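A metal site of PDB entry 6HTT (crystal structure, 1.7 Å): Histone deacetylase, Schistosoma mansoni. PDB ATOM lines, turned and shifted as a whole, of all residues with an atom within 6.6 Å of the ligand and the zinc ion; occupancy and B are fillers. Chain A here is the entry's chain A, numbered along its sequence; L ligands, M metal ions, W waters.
The side-chain hydroxyl (OH) of Tyr 342 lies close to an oxygen (O3) of the ligand, at 2.4 Å. A ring nitrogen (NE2) of His 142 sits close to an oxygen (O1) of the ligand, at 2.7 Å. NE2 of His 143 is in hydrogen-bond range of N2 of the ligand. A ring nitrogen (NE2) of His 293 sits at hydrogen-bond distance from a nitrogen (N1) of the ligand, 2.8 Å away. The side-chain amino group (NZ) of Lys 21 lies within hydrogen-bond range of an oxygen (O2) of the ligand, 3.1 Å away.
NE2 of Gln 282 lies within hydrogen-bond range of OD2 of Asp 187 (3.0 Å). N of Leu 188 sits at hydrogen-bond distance from OD1 of Asp 286. The backbone NH of Tyr 342 sits at hydrogen-bond distance from the side-chain carboxylate of Asp 291, at 2.9 Å. NE2 of His 143 is in hydrogen-bond range of NE2 of His 142, at 3.1 Å. SG of Cys 153 lies within hydrogen-bond range of N of His 142 (3.8 Å). SG of Cys 153 sits at hydrogen-bond distance from N of His 143 (3.5 Å). OD1 of Asp 291 lies within hydrogen-bond range of N of His 293. The backbone carbonyl oxygen of Gly 151 lies within hydrogen-bond range of the side-chain sulfur of Cys 153 (3.6 Å).
Residues that only touch the ligand: Pro 292 (3.6 Å), Phe 217 (3.6 Å), Gly 340 (3.8 Å) and Gly 151 (3.9 Å). Hydrophobic or aromatic side chains within 4 Å of the ligand: His 142, His 143, His 189, Phe 217, Pro 292, His 293 and Tyr 342. Of the 25 residues printed, 12 come within 4 Å of the ligand. The nearest printed residue that does not touch the ligand is Asp 101 (4.8 Å).
Three residues have an atom within 4 Å of the zinc ion: Asp 187, His 189 and Asp 286.
The zinc ion is bound by the side-chain carboxylate of Asp 187, the side-chain carboxylate of Asp 286, a ring nitrogen (ND1) of His 189, an oxygen (O3) of the ligand and an oxygen (O1) of the ligand.
Water W1 lies within hydrogen-bond range of N of Gly 340 (3.3 Å), NE2 of His 142 (3.4 Å) and N2 of the ligand (3.5 Å).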
ATOM      1  N   LYS A  21     -24.490  29.899   0.505  1.00  0.00           N
ATOM      2  CA  LYS A  21     -24.149  30.196  -0.879  1.00  0.00           C
ATOM      3  C   LYS A  21     -25.141  31.171  -1.511  1.00  0.00           C
ATOM      4  O   LYS A  21     -24.743  32.076  -2.255  1.00  0.00           O
ATOM      5  CB  LYS A  21     -24.088  28.907  -1.705  1.00  0.00           C
ATOM      6  CG  LYS A  21     -23.528  29.164  -3.108  1.00  0.00           C
ATOM      7  CD  LYS A  21     -22.804  27.958  -3.675  1.00  0.00           C
ATOM      8  CE  LYS A  21     -21.966  28.343  -4.895  1.00  0.00           C
ATOM      9  NZ  LYS A  21     -20.960  29.414  -4.598  1.00  0.00           N
ATOM     10  N   PHE A  22     -26.438  31.002  -1.243  1.00  0.00           N
ATOM     11  CA  PHE A  22     -27.430  31.823  -1.933  1.00  0.00           C
ATOM     12  C   PHE A  22     -27.970  32.949  -1.058  1.00  0.00           C
ATOM     13  O   PHE A  22     -28.752  33.762  -1.557  1.00  0.00           O
ATOM     14  CB  PHE A  22     -28.552  30.940  -2.485  1.00  0.00           C
ATOM     15  CG  PHE A  22     -28.098  30.120  -3.668  1.00  0.00           C
ATOM     16  CD1 PHE A  22     -27.988  30.707  -4.924  1.00  0.00           C
ATOM     17  CD2 PHE A  22     -27.699  28.798  -3.516  1.00  0.00           C
ATOM     18  CE1 PHE A  22     -27.533  29.967  -6.019  1.00  0.00           C
ATOM     19  CE2 PHE A  22     -27.239  28.061  -4.603  1.00  0.00           C
ATOM     20  CZ  PHE A  22     -27.160  28.650  -5.854  1.00  0.00           C
ATOM     21  N   ASP A 101     -17.862  21.700  -1.757  1.00  0.00           N
ATOM     22  CA  ASP A 101     -18.804  22.702  -2.270  1.00  0.00           C
ATOM     23  C   ASP A 101     -20.248  22.436  -1.870  1.00  0.00           C
ATOM     24  O   ASP A 101     -21.105  23.272  -2.155  1.00  0.00           O
ATOM     25  CB  ASP A 101     -18.701  22.802  -3.795  1.00  0.00           C
ATOM     26  CG  ASP A 101     -17.510  23.629  -4.250  1.00  0.00           C
ATOM     27  OD1 ASP A 101     -16.697  24.004  -3.382  1.00  0.00           O
ATOM     28  OD2 ASP A 101     -17.397  23.909  -5.466  1.00  0.00           O
ATOM     29  N   GLY A 140     -35.257  24.486  -8.643  1.00  0.00           N
ATOM     30  CA  GLY A 140     -34.407  24.341  -9.811  1.00  0.00           C
ATOM     31  C   GLY A 140     -33.026  23.769  -9.567  1.00  0.00           C
ATOM     32  O   GLY A 140     -32.088  24.127 -10.298  1.00  0.00           O
ATOM     33  N   HIS A 142     -30.624  21.338 -10.138  1.00  0.00           N
ATOM     34  CA  HIS A 142     -30.568  20.288 -11.144  1.00  0.00           C
ATOM     35  C   HIS A 142     -29.394  19.323 -10.990  1.00  0.00           C
ATOM     36  O   HIS A 142     -29.372  18.307 -11.676  1.00  0.00           O
ATOM     37  CB  HIS A 142     -30.552  20.905 -12.566  1.00  0.00           C
ATOM     38  CG  HIS A 142     -29.432  21.869 -12.820  1.00  0.00           C
ATOM     39  ND1 HIS A 142     -29.202  22.418 -14.066  1.00  0.00           N
ATOM     40  CD2 HIS A 142     -28.507  22.419 -12.001  1.00  0.00           C
ATOM     41  CE1 HIS A 142     -28.166  23.239 -14.010  1.00  0.00           C
ATOM     42  NE2 HIS A 142     -27.724  23.263 -12.760  1.00  0.00           N
ATOM     43  N   HIS A 143     -28.443  19.581 -10.090  1.00  0.00           N
ATOM     44  CA  HIS A 143     -27.228  18.743 -10.023  1.00  0.00           C
ATOM     45  C   HIS A 143     -27.336  17.556  -9.068  1.00  0.00           C
ATOM     46  O   HIS A 143     -26.521  16.636  -9.173  1.00  0.00           O
ATOM     47  CB  HIS A 143     -26.026  19.576  -9.591  1.00  0.00           C
ATOM     48  CG  HIS A 143     -25.597  20.588 -10.601  1.00  0.00           C
ATOM     49  ND1 HIS A 143     -25.392  20.272 -11.927  1.00  0.00           N
ATOM     50  CD2 HIS A 143     -25.306  21.913 -10.478  1.00  0.00           C
ATOM     51  CE1 HIS A 143     -24.992  21.357 -12.576  1.00  0.00           C
ATOM     52  NE2 HIS A 143     -24.929  22.354 -11.723  1.00  0.00           N
ATOM     53  N   SER A 150     -24.283  17.751  -5.149  1.00  0.00           N
ATOM     54  CA  SER A 150     -23.359  18.226  -6.174  1.00  0.00           C
ATOM     55  C   SER A 150     -23.686  19.683  -6.470  1.00  0.00           C
ATOM     56  O   SER A 150     -24.849  20.030  -6.631  1.00  0.00           O
ATOM     57  CB  SER A 150     -23.481  17.386  -7.434  1.00  0.00           C
ATOM     58  OG  SER A 150     -22.642  17.912  -8.469  1.00  0.00           O
ATOM     59  N   GLY A 151     -22.651  20.518  -6.564  1.00  0.00           N
ATOM     60  CA  GLY A 151     -22.872  21.885  -7.026  1.00  0.00           C
ATOM     61  C   GLY A 151     -23.865  22.682  -6.193  1.00  0.00           C
ATOM     62  O   GLY A 151     -24.701  23.407  -6.748  1.00  0.00           O
ATOM     63  N   PHE A 152     -23.785  22.555  -4.866  1.00  0.00           N
ATOM     64  CA  PHE A 152     -24.702  23.153  -3.885  1.00  0.00           C
ATOM     65  C   PHE A 152     -26.162  22.759  -4.113  1.00  0.00           C
ATOM     66  O   PHE A 152     -27.075  23.459  -3.647  1.00  0.00           O
ATOM     67  CB  PHE A 152     -24.576  24.683  -3.816  1.00  0.00           C
ATOM     68  CG  PHE A 152     -24.928  25.234  -2.445  1.00  0.00           C
ATOM     69  CD1 PHE A 152     -24.013  25.167  -1.416  1.00  0.00           C
ATOM     70  CD2 PHE A 152     -26.196  25.763  -2.187  1.00  0.00           C
ATOM     71  CE1 PHE A 152     -24.326  25.635  -0.142  1.00  0.00           C
ATOM     72  CE2 PHE A 152     -26.518  26.233  -0.934  1.00  0.00           C
ATOM     73  CZ  PHE A 152     -25.576  26.179   0.099  1.00  0.00           C
ATOM     74  N   CYS A 153     -26.377  21.632  -4.782  1.00  0.00           N
ATOM     75  CA  CYS A 153     -27.690  21.008  -4.912  1.00  0.00           C
ATOM     76  C   CYS A 153     -27.713  19.784  -4.024  1.00  0.00           C
ATOM     77  O   CYS A 153     -26.889  18.874  -4.211  1.00  0.00           O
ATOM     78  CB  CYS A 153     -27.968  20.614  -6.378  1.00  0.00           C
ATOM     79  SG  CYS A 153     -27.972  21.999  -7.535  1.00  0.00           S
ATOM     80  N   ASP A 187     -29.875  26.914 -17.629  1.00  0.00           N
ATOM     81  CA  ASP A 187     -28.762  27.268 -16.759  1.00  0.00           C
ATOM     82  C   ASP A 187     -27.450  27.277 -17.551  1.00  0.00           C
ATOM     83  O   ASP A 187     -27.312  26.614 -18.589  1.00  0.00           O
ATOM     84  CB  ASP A 187     -28.681  26.256 -15.615  1.00  0.00           C
ATOM     85  CG  ASP A 187     -27.853  26.724 -14.442  1.00  0.00           C
ATOM     86  OD1 ASP A 187     -26.615  26.583 -14.491  1.00  0.00           O
ATOM     87  OD2 ASP A 187     -28.457  27.156 -13.443  1.00  0.00           O
ATOM     88  N   LEU A 188     -26.484  28.043 -17.047  1.00  0.00           N
ATOM     89  CA  LEU A 188     -25.136  28.020 -17.628  1.00  0.00           C
ATOM     90  C   LEU A 188     -24.531  26.632 -17.584  1.00  0.00           C
ATOM     91  O   LEU A 188     -23.716  26.275 -18.427  1.00  0.00           O
ATOM     92  CB  LEU A 188     -24.236  28.997 -16.872  1.00  0.00           C
ATOM     93  CG  LEU A 188     -22.788  29.087 -17.359  1.00  0.00           C
ATOM     94  CD1 LEU A 188     -22.719  29.719 -18.744  1.00  0.00           C
ATOM     95  CD2 LEU A 188     -21.965  29.895 -16.360  1.00  0.00           C
ATOM     96  N   HIS A 189     -24.920  25.836 -16.599  1.00  0.00           N
ATOM     97  CA  HIS A 189     -24.342  24.521 -16.377  1.00  0.00           C
ATOM     98  C   HIS A 189     -25.227  23.411 -16.929  1.00  0.00           C
ATOM     99  O   HIS A 189     -26.457  23.535 -16.975  1.00  0.00           O
ATOM    100  CB  HIS A 189     -24.105  24.279 -14.883  1.00  0.00           C
ATOM    101  CG  HIS A 189     -23.144  25.258 -14.282  1.00  0.00           C
ATOM    102  ND1 HIS A 189     -23.554  26.445 -13.708  1.00  0.00           N
ATOM    103  CD2 HIS A 189     -21.797  25.265 -14.233  1.00  0.00           C
ATOM    104  CE1 HIS A 189     -22.491  27.121 -13.293  1.00  0.00           C
ATOM    105  NE2 HIS A 189     -21.403  26.420 -13.601  1.00  0.00           N
ATOM    106  N   HIS A 190     -24.579  22.311 -17.317  1.00  0.00           N
ATOM    107  CA  HIS A 190     -25.304  21.117 -17.754  1.00  0.00           C
ATOM    108  C   HIS A 190     -26.210  20.590 -16.645  1.00  0.00           C
ATOM    109  O   HIS A 190     -25.786  20.411 -15.496  1.00  0.00           O
ATOM    110  CB  HIS A 190     -24.306  20.047 -18.175  1.00  0.00           C
ATOM    111  CG  HIS A 190     -24.960  18.756 -18.586  1.00  0.00           C
ATOM    112  ND1 HIS A 190     -24.613  17.542 -18.038  1.00  0.00           N
ATOM    113  CD2 HIS A 190     -25.969  18.512 -19.449  1.00  0.00           C
ATOM    114  CE1 HIS A 190     -25.359  16.590 -18.572  1.00  0.00           C
ATOM    115  NE2 HIS A 190     -26.201  17.148 -19.430  1.00  0.00           N
ATOM    116  N   PHE A 217     -17.369  22.835 -14.687  1.00  0.00           N
ATOM    117  CA  PHE A 217     -18.358  22.017 -13.971  1.00  0.00           C
ATOM    118  C   PHE A 217     -19.649  21.826 -14.786  1.00  0.00           C
ATOM    119  O   PHE A 217     -20.113  22.774 -15.428  1.00  0.00           O
ATOM    120  CB  PHE A 217     -18.651  22.698 -12.625  1.00  0.00           C
ATOM    121  CG  PHE A 217     -19.559  21.922 -11.728  1.00  0.00           C
ATOM    122  CD1 PHE A 217     -20.931  22.102 -11.767  1.00  0.00           C
ATOM    123  CD2 PHE A 217     -19.031  21.007 -10.819  1.00  0.00           C
ATOM    124  CE1 PHE A 217     -21.767  21.377 -10.930  1.00  0.00           C
ATOM    125  CE2 PHE A 217     -19.863  20.284  -9.974  1.00  0.00           C
ATOM    126  CZ  PHE A 217     -21.231  20.469 -10.030  1.00  0.00           C
ATOM    127  N   GLN A 282     -35.887  25.002 -16.280  1.00  0.00           N
ATOM    128  CA  GLN A 282     -34.948  25.512 -15.294  1.00  0.00           C
ATOM    129  C   GLN A 282     -34.378  26.797 -15.875  1.00  0.00           C
ATOM    130  O   GLN A 282     -33.863  26.798 -17.004  1.00  0.00           O
ATOM    131  CB  GLN A 282     -33.872  24.453 -15.000  1.00  0.00           C
ATOM    132  CG  GLN A 282     -33.090  24.671 -13.725  1.00  0.00           C
ATOM    133  CD  GLN A 282     -31.849  25.503 -13.931  1.00  0.00           C
ATOM    134  OE1 GLN A 282     -31.760  26.237 -14.908  1.00  0.00           O
ATOM    135  NE2 GLN A 282     -30.894  25.391 -13.014  1.00  0.00           N
ATOM    136  N   GLY A 284     -31.966  29.039 -14.585  1.00  0.00           N
ATOM    137  CA  GLY A 284     -30.791  29.560 -13.914  1.00  0.00           C
ATOM    138  C   GLY A 284     -30.248  30.799 -14.608  1.00  0.00           C
ATOM    139  O   GLY A 284     -30.095  30.819 -15.825  1.00  0.00           O
ATOM    140  N   ASP A 286     -27.301  32.266 -14.418  1.00  0.00           N
ATOM    141  CA  ASP A 286     -25.856  32.439 -14.490  1.00  0.00           C
ATOM    142  C   ASP A 286     -25.327  32.589 -15.917  1.00  0.00           C
ATOM    143  O   ASP A 286     -24.111  32.699 -16.092  1.00  0.00           O
ATOM    144  CB  ASP A 286     -25.092  31.294 -13.773  1.00  0.00           C
ATOM    145  CG  ASP A 286     -25.763  29.934 -13.905  1.00  0.00           C
ATOM    146  OD1 ASP A 286     -26.692  29.737 -14.733  1.00  0.00           O
ATOM    147  OD2 ASP A 286     -25.298  29.037 -13.163  1.00  0.00           O
ATOM    148  N   ASP A 291     -23.166  37.887 -14.528  1.00  0.00           N
ATOM    149  CA  ASP A 291     -22.929  36.842 -13.541  1.00  0.00           C
ATOM    150  C   ASP A 291     -21.430  36.738 -13.263  1.00  0.00           C
ATOM    151  O   ASP A 291     -20.618  36.927 -14.170  1.00  0.00           O
ATOM    152  CB  ASP A 291     -23.480  35.510 -14.027  1.00  0.00           C
ATOM    153  CG  ASP A 291     -23.484  34.476 -12.937  1.00  0.00           C
ATOM    154  OD1 ASP A 291     -22.430  33.830 -12.740  1.00  0.00           O
ATOM    155  OD2 ASP A 291     -24.529  34.351 -12.244  1.00  0.00           O
ATOM    156  N   PRO A 292     -21.029  36.446 -12.019  1.00  0.00           N
ATOM    157  CA  PRO A 292     -19.584  36.316 -11.725  1.00  0.00           C
ATOM    158  C   PRO A 292     -18.888  35.204 -12.510  1.00  0.00           C
ATOM    159  O   PRO A 292     -17.658  35.251 -12.655  1.00  0.00           O
ATOM    160  CB  PRO A 292     -19.531  36.034 -10.223  1.00  0.00           C
ATOM    161  CG  PRO A 292     -20.916  36.186  -9.700  1.00  0.00           C
ATOM    162  CD  PRO A 292     -21.885  36.312 -10.820  1.00  0.00           C
ATOM    163  N   HIS A 293     -19.634  34.215 -13.030  1.00  0.00           N
ATOM    164  CA  HIS A 293     -19.023  33.248 -13.937  1.00  0.00           C
ATOM    165  C   HIS A 293     -18.407  33.927 -15.154  1.00  0.00           C
ATOM    166  O   HIS A 293     -17.355  33.495 -15.649  1.00  0.00           O
ATOM    167  CB  HIS A 293     -20.056  32.234 -14.387  1.00  0.00           C
ATOM    168  CG  HIS A 293     -20.311  31.154 -13.383  1.00  0.00           C
ATOM    169  ND1 HIS A 293     -19.473  30.062 -13.249  1.00  0.00           N
ATOM    170  CD2 HIS A 293     -21.288  30.994 -12.458  1.00  0.00           C
ATOM    171  CE1 HIS A 293     -19.933  29.282 -12.280  1.00  0.00           C
ATOM    172  NE2 HIS A 293     -21.034  29.819 -11.790  1.00  0.00           N
ATOM    173  N   GLY A 339     -32.612  28.336 -10.182  1.00  0.00           N
ATOM    174  CA  GLY A 339     -31.354  27.604 -10.328  1.00  0.00           C
ATOM    175  C   GLY A 339     -30.174  28.533 -10.007  1.00  0.00           C
ATOM    176  O   GLY A 339     -30.236  29.325  -9.075  1.00  0.00           O
ATOM    177  N   GLY A 340     -29.112  28.392 -10.795  1.00  0.00           N
ATOM    178  CA  GLY A 340     -27.951  29.247 -10.604  1.00  0.00           C
ATOM    179  C   GLY A 340     -28.287  30.712 -10.801  1.00  0.00           C
ATOM    180  O   GLY A 340     -29.365  31.109 -11.234  1.00  0.00           O
ATOM    181  N   GLY A 341     -27.300  31.548 -10.471  1.00  0.00           N
ATOM    182  CA  GLY A 341     -27.421  32.992 -10.559  1.00  0.00           C
ATOM    183  C   GLY A 341     -26.758  33.635  -9.356  1.00  0.00           C
ATOM    184  O   GLY A 341     -27.345  33.658  -8.271  1.00  0.00           O
ATOM    185  N   TYR A 342     -25.550  34.148  -9.523  1.00  0.00           N
ATOM    186  CA  TYR A 342     -24.714  34.524  -8.390  1.00  0.00           C
ATOM    187  C   TYR A 342     -24.521  36.026  -8.310  1.00  0.00           C
ATOM    188  O   TYR A 342     -23.868  36.506  -7.373  1.00  0.00           O
ATOM    189  CB  TYR A 342     -23.392  33.741  -8.476  1.00  0.00           C
ATOM    190  CG  TYR A 342     -23.759  32.270  -8.559  1.00  0.00           C
ATOM    191  CD1 TYR A 342     -24.075  31.564  -7.408  1.00  0.00           C
ATOM    192  CD2 TYR A 342     -23.908  31.636  -9.792  1.00  0.00           C
ATOM    193  CE1 TYR A 342     -24.486  30.240  -7.478  1.00  0.00           C
ATOM    194  CE2 TYR A 342     -24.319  30.330  -9.869  1.00  0.00           C
ATOM    195  CZ  TYR A 342     -24.603  29.631  -8.702  1.00  0.00           C
ATOM    196  OH  TYR A 342     -25.001  28.326  -8.775  1.00  0.00           O
HETATM  197  C1  LIG L   1     -22.883  26.026 -10.031  1.00  0.00           C
HETATM  198  C2  LIG L   1     -22.216  27.162  -9.576  1.00  0.00           C
HETATM  199  C3  LIG L   1     -21.016  27.056  -8.880  1.00  0.00           C
HETATM  200  C4  LIG L   1     -20.469  25.788  -8.649  1.00  0.00           C
HETATM  201  C5  LIG L   1     -21.122  24.653  -9.100  1.00  0.00           C
HETATM  202  C6  LIG L   1     -24.168  26.165 -10.779  1.00  0.00           C
HETATM  203  O1  LIG L   1     -25.914  25.152 -11.966  1.00  0.00           O
HETATM  204  C7  LIG L   1     -20.450  31.344  -7.613  1.00  0.00           C
HETATM  205  C8  LIG L   1     -19.954  30.673  -8.723  1.00  0.00           C
HETATM  206  C9  LIG L   1     -18.966  31.274  -9.495  1.00  0.00           C
HETATM  207  C10 LIG L   1     -18.492  32.532  -9.166  1.00  0.00           C
HETATM  208  C11 LIG L   1     -18.997  33.196  -8.073  1.00  0.00           C
HETATM  209  C12 LIG L   1     -19.971  32.606  -7.301  1.00  0.00           C
HETATM  210  N1  LIG L   1     -20.451  29.398  -9.068  1.00  0.00           N
HETATM  211  C13 LIG L   1     -20.371  28.280  -8.316  1.00  0.00           C
HETATM  212  C14 LIG L   1     -22.322  24.768  -9.775  1.00  0.00           C
HETATM  213  N2  LIG L   1     -24.709  25.059 -11.266  1.00  0.00           N
HETATM  214  O2  LIG L   1     -19.827  28.255  -7.212  1.00  0.00           O
HETATM  215  O3  LIG L   1     -24.693  27.266 -10.942  1.00  0.00           O
HETATM  216 ZN    ZN M   1     -25.438  27.068 -12.984  1.00  0.00          ZN
HETATM  217  O   HOH W   1     -27.983  25.367 -10.078  1.00  0.00           O
